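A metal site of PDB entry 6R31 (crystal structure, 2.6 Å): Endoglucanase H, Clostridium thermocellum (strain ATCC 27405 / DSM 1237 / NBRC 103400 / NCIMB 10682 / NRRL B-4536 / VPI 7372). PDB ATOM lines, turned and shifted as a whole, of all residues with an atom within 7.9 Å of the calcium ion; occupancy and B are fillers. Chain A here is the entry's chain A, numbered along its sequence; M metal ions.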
ATOM      1  N   MET A   9     -23.609  18.996  35.002  1.00  0.00           N
ATOM      2  CA  MET A   9     -23.183  19.424  33.676  1.00  0.00           C
ATOM      3  C   MET A   9     -24.331  20.084  32.935  1.00  0.00           C
ATOM      4  O   MET A   9     -25.374  19.467  32.767  1.00  0.00           O
ATOM      5  CB  MET A   9     -22.698  18.218  32.854  1.00  0.00           C
ATOM      6  CG  MET A   9     -22.243  18.550  31.436  1.00  0.00           C
ATOM      7  SD  MET A   9     -20.526  19.161  31.359  1.00  0.00           S
ATOM      8  CE  MET A   9     -19.607  17.664  31.687  1.00  0.00           C
ATOM      9  N   ASP A  11     -23.625  21.767  29.628  1.00  0.00           N
ATOM     10  CA  ASP A  11     -23.331  21.535  28.225  1.00  0.00           C
ATOM     11  C   ASP A  11     -21.896  21.047  28.047  1.00  0.00           C
ATOM     12  O   ASP A  11     -20.930  21.763  28.331  1.00  0.00           O
ATOM     13  CB  ASP A  11     -23.623  22.780  27.359  1.00  0.00           C
ATOM     14  CG  ASP A  11     -24.132  22.482  25.960  1.00  0.00           C
ATOM     15  OD1 ASP A  11     -23.640  21.507  25.358  1.00  0.00           O
ATOM     16  OD2 ASP A  11     -25.028  23.212  25.482  1.00  0.00           O
ATOM     17  N   ASP A  12     -21.764  19.797  27.586  1.00  0.00           N
ATOM     18  CA  ASP A  12     -20.501  19.192  27.219  1.00  0.00           C
ATOM     19  C   ASP A  12     -20.342  19.234  25.697  1.00  0.00           C
ATOM     20  O   ASP A  12     -19.285  18.888  25.172  1.00  0.00           O
ATOM     21  CB  ASP A  12     -20.403  17.764  27.777  1.00  0.00           C
ATOM     22  CG  ASP A  12     -21.540  16.834  27.366  1.00  0.00           C
ATOM     23  OD1 ASP A  12     -22.416  17.254  26.585  1.00  0.00           O
ATOM     24  OD2 ASP A  12     -21.540  15.687  27.845  1.00  0.00           O
ATOM     25  N   PHE A  13     -21.414  19.639  24.996  1.00  0.00           N
ATOM     26  CA  PHE A  13     -21.394  19.876  23.556  1.00  0.00           C
ATOM     27  C   PHE A  13     -21.263  18.561  22.793  1.00  0.00           C
ATOM     28  O   PHE A  13     -20.589  18.486  21.770  1.00  0.00           O
ATOM     29  CB  PHE A  13     -20.306  20.881  23.179  1.00  0.00           C
ATOM     30  CG  PHE A  13     -20.623  22.265  23.670  1.00  0.00           C
ATOM     31  CD1 PHE A  13     -21.516  23.081  22.996  1.00  0.00           C
ATOM     32  CD2 PHE A  13     -20.088  22.723  24.866  1.00  0.00           C
ATOM     33  CE1 PHE A  13     -21.844  24.332  23.480  1.00  0.00           C
ATOM     34  CE2 PHE A  13     -20.411  23.979  25.343  1.00  0.00           C
ATOM     35  CZ  PHE A  13     -21.287  24.780  24.656  1.00  0.00           C
ATOM     36  N   GLU A  14     -21.939  17.530  23.292  1.00  0.00           N
ATOM     37  CA  GLU A  14     -21.925  16.222  22.658  1.00  0.00           C
ATOM     38  C   GLU A  14     -23.295  15.937  22.049  1.00  0.00           C
ATOM     39  O   GLU A  14     -23.490  14.892  21.429  1.00  0.00           O
ATOM     40  CB  GLU A  14     -21.525  15.137  23.672  1.00  0.00           C
ATOM     41  CG  GLU A  14     -20.283  15.472  24.480  1.00  0.00           C
ATOM     42  CD  GLU A  14     -18.976  15.555  23.693  1.00  0.00           C
ATOM     43  OE1 GLU A  14     -18.879  14.872  22.638  1.00  0.00           O
ATOM     44  OE2 GLU A  14     -18.064  16.304  24.121  1.00  0.00           O
ATOM     45  N   GLY A  15     -24.249  16.862  22.231  1.00  0.00           N
ATOM     46  CA  GLY A  15     -25.661  16.571  21.987  1.00  0.00           C
ATOM     47  C   GLY A  15     -26.382  17.683  21.226  1.00  0.00           C
ATOM     48  O   GLY A  15     -25.932  18.118  20.168  1.00  0.00           O
ATOM     49  N   VAL A  34     -16.653  21.934  17.044  1.00  0.00           N
ATOM     50  CA  VAL A  34     -15.287  21.539  16.721  1.00  0.00           C
ATOM     51  C   VAL A  34     -14.757  20.623  17.823  1.00  0.00           C
ATOM     52  O   VAL A  34     -15.409  20.457  18.862  1.00  0.00           O
ATOM     53  CB  VAL A  34     -14.337  22.747  16.549  1.00  0.00           C
ATOM     54  CG1 VAL A  34     -14.749  23.660  15.400  1.00  0.00           C
ATOM     55  CG2 VAL A  34     -14.177  23.563  17.829  1.00  0.00           C
ATOM     56  N   SER A  35     -13.564  20.044  17.587  1.00  0.00           N
ATOM     57  CA  SER A  35     -12.816  19.361  18.632  1.00  0.00           C
ATOM     58  C   SER A  35     -12.707  20.284  19.838  1.00  0.00           C
ATOM     59  O   SER A  35     -12.135  21.358  19.722  1.00  0.00           O
ATOM     60  CB  SER A  35     -11.453  18.956  18.144  1.00  0.00           C
ATOM     61  OG  SER A  35     -11.551  17.963  17.153  1.00  0.00           O
ATOM     62  N   GLY A  36     -13.292  19.875  20.959  1.00  0.00           N
ATOM     63  CA  GLY A  36     -13.291  20.657  22.187  1.00  0.00           C
ATOM     64  C   GLY A  36     -12.186  20.175  23.124  1.00  0.00           C
ATOM     65  O   GLY A  36     -11.195  19.601  22.674  1.00  0.00           O
ATOM     66  N   LYS A  37     -12.371  20.402  24.435  1.00  0.00           N
ATOM     67  CA  LYS A  37     -11.374  19.994  25.415  1.00  0.00           C
ATOM     68  C   LYS A  37     -11.474  18.488  25.674  1.00  0.00           C
ATOM     69  O   LYS A  37     -10.445  17.828  25.801  1.00  0.00           O
ATOM     70  CB  LYS A  37     -11.424  20.818  26.702  1.00  0.00           C
ATOM     71  CG  LYS A  37     -10.249  20.581  27.644  1.00  0.00           C
ATOM     72  CD  LYS A  37     -10.326  21.367  28.931  1.00  0.00           C
ATOM     73  CE  LYS A  37      -9.299  20.940  29.958  1.00  0.00           C
ATOM     74  NZ  LYS A  37      -9.509  19.533  30.392  1.00  0.00           N
ATOM     75  N   THR A  38     -12.698  17.961  25.789  1.00  0.00           N
ATOM     76  CA  THR A  38     -12.943  16.529  25.619  1.00  0.00           C
ATOM     77  C   THR A  38     -14.107  16.308  24.650  1.00  0.00           C
ATOM     78  O   THR A  38     -15.159  16.936  24.765  1.00  0.00           O
ATOM     79  CB  THR A  38     -13.100  15.801  26.960  1.00  0.00           C
ATOM     80  OG1 THR A  38     -13.890  16.593  27.836  1.00  0.00           O
ATOM     81  CG2 THR A  38     -11.791  15.476  27.644  1.00  0.00           C
ATOM     82  N   GLY A  39     -13.907  15.401  23.697  1.00  0.00           N
ATOM     83  CA  GLY A  39     -14.806  15.293  22.563  1.00  0.00           C
ATOM     84  C   GLY A  39     -14.911  16.648  21.878  1.00  0.00           C
ATOM     85  O   GLY A  39     -13.899  17.271  21.543  1.00  0.00           O
ATOM     86  N   ASN A  40     -16.148  17.123  21.737  1.00  0.00           N
ATOM     87  CA  ASN A  40     -16.454  18.294  20.924  1.00  0.00           C
ATOM     88  C   ASN A  40     -16.812  19.473  21.821  1.00  0.00           C
ATOM     89  O   ASN A  40     -17.363  19.301  22.906  1.00  0.00           O
ATOM     90  CB  ASN A  40     -17.629  18.013  20.004  1.00  0.00           C
ATOM     91  CG  ASN A  40     -17.230  17.197  18.794  1.00  0.00           C
ATOM     92  OD1 ASN A  40     -16.053  17.125  18.439  1.00  0.00           O
ATOM     93  ND2 ASN A  40     -18.207  16.585  18.156  1.00  0.00           N
ATOM     94  N   GLY A  41     -16.504  20.673  21.314  1.00  0.00           N
ATOM     95  CA  GLY A  41     -16.873  21.919  21.955  1.00  0.00           C
ATOM     96  C   GLY A  41     -17.393  22.899  20.910  1.00  0.00           C
ATOM     97  O   GLY A  41     -17.504  22.545  19.736  1.00  0.00           O
ATOM     98  N   MET A  42     -17.677  24.131  21.332  1.00  0.00           N
ATOM     99  CA  MET A  42     -18.288  25.106  20.451  1.00  0.00           C
ATOM    100  C   MET A  42     -17.310  26.246  20.152  1.00  0.00           C
ATOM    101  O   MET A  42     -16.887  26.980  21.045  1.00  0.00           O
ATOM    102  CB  MET A  42     -19.561  25.681  21.057  1.00  0.00           C
ATOM    103  CG  MET A  42     -20.080  26.880  20.300  1.00  0.00           C
ATOM    104  SD  MET A  42     -21.667  27.435  20.911  1.00  0.00           S
ATOM    105  CE  MET A  42     -21.186  28.309  22.410  1.00  0.00           C
ATOM    106  N   ASP A  74     -14.534  25.267  30.387  1.00  0.00           N
ATOM    107  CA  ASP A  74     -13.221  25.251  29.755  1.00  0.00           C
ATOM    108  C   ASP A  74     -13.216  26.154  28.515  1.00  0.00           C
ATOM    109  O   ASP A  74     -14.081  25.993  27.661  1.00  0.00           O
ATOM    110  CB  ASP A  74     -12.811  23.836  29.381  1.00  0.00           C
ATOM    111  CG  ASP A  74     -12.799  22.877  30.559  1.00  0.00           C
ATOM    112  OD1 ASP A  74     -12.435  23.326  31.669  1.00  0.00           O
ATOM    113  OD2 ASP A  74     -13.158  21.693  30.374  1.00  0.00           O
ATOM    114  N   VAL A 162     -15.180  26.747  23.556  1.00  0.00           N
ATOM    115  CA  VAL A 162     -15.609  26.439  24.912  1.00  0.00           C
ATOM    116  C   VAL A 162     -16.005  24.966  25.006  1.00  0.00           C
ATOM    117  O   VAL A 162     -16.265  24.333  23.984  1.00  0.00           O
ATOM    118  CB  VAL A 162     -16.723  27.359  25.465  1.00  0.00           C
ATOM    119  CG1 VAL A 162     -16.259  28.802  25.593  1.00  0.00           C
ATOM    120  CG2 VAL A 162     -18.014  27.260  24.687  1.00  0.00           C
ATOM    121  N   ASP A 163     -16.047  24.453  26.244  1.00  0.00           N
ATOM    122  CA  ASP A 163     -16.363  23.062  26.541  1.00  0.00           C
ATOM    123  C   ASP A 163     -16.663  22.903  28.026  1.00  0.00           C
ATOM    124  O   ASP A 163     -16.220  23.706  28.854  1.00  0.00           O
ATOM    125  CB  ASP A 163     -15.218  22.138  26.097  1.00  0.00           C
ATOM    126  CG  ASP A 163     -15.629  20.688  25.933  1.00  0.00           C
ATOM    127  OD1 ASP A 163     -16.847  20.400  26.022  1.00  0.00           O
ATOM    128  OD2 ASP A 163     -14.740  19.855  25.700  1.00  0.00           O
ATOM    129  N   ASN A 164     -17.452  21.868  28.334  1.00  0.00           N
ATOM    130  CA  ASN A 164     -17.743  21.366  29.673  1.00  0.00           C
ATOM    131  C   ASN A 164     -18.255  22.460  30.623  1.00  0.00           C
ATOM    132  O   ASN A 164     -17.659  22.719  31.671  1.00  0.00           O
ATOM    133  CB  ASN A 164     -16.600  20.519  30.221  1.00  0.00           C
ATOM    134  CG  ASN A 164     -16.218  19.404  29.271  1.00  0.00           C
ATOM    135  OD1 ASN A 164     -17.038  18.558  28.908  1.00  0.00           O
ATOM    136  ND2 ASN A 164     -14.964  19.396  28.831  1.00  0.00           N
ATOM    137  N   ILE A 165     -19.395  23.055  30.269  1.00  0.00           N
ATOM    138  CA  ILE A 165     -20.055  24.051  31.095  1.00  0.00           C
ATOM    139  C   ILE A 165     -20.916  23.353  32.138  1.00  0.00           C
ATOM    140  O   ILE A 165     -21.824  22.591  31.783  1.00  0.00           O
ATOM    141  CB  ILE A 165     -20.902  24.985  30.216  1.00  0.00           C
ATOM    142  CG1 ILE A 165     -20.187  25.326  28.912  1.00  0.00           C
ATOM    143  CG2 ILE A 165     -21.355  26.213  31.005  1.00  0.00           C
ATOM    144  CD1 ILE A 165     -20.567  26.643  28.259  1.00  0.00           C
HETATM  145 CA    CA M   1     -17.089  17.992  25.158  1.00  0.00          CA
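O of Asp 163 sits at hydrogen-bond distance from N of Asp 74.
The backbone NH (N) of Asn 164 is in hydrogen-bond range of the backbone carbonyl oxygen (O) of Asp 11.
The side-chain carboxylate of Asp 163 is in hydrogen-bond range of the backbone NH of Lys 37 (2.7 Å).
The side-chain carboxylate of Asp 163 is in hydrogen-bond range of the side-chain amide nitrogen of Asn 164 (3.2 Å).
ND2 of Asn 164 is in hydrogen-bond range of OD2 of Asp 74, 3.3 Å away.
OG1 of Thr 38 is in hydrogen-bond range of ND2 of Asn 164.
OD1 of Asn 40 lies close to O of Val 34 (3.4 Å).
Residues that only touch the calcium ion: Asn 164.
Within 4 Å of the calcium ion: Asp 12, Glu 14, Thr 38, Asn 40, Asp 163 and Asn 164.
The calcium ion is bound by OE2 of Glu 14 (2.2 Å), O of Thr 38 (2.2 Å), O of Asp 12 (2.4 Å), OD1 of Asp 163 (2.6 Å) and O of Asn 40 (2.6 Å).
The calcium ion has five donor atoms within binding distance.
Slightly farther from the calcium ion lies the side-chain carboxylate (OD2) of Asp 163 (3.0 Å).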
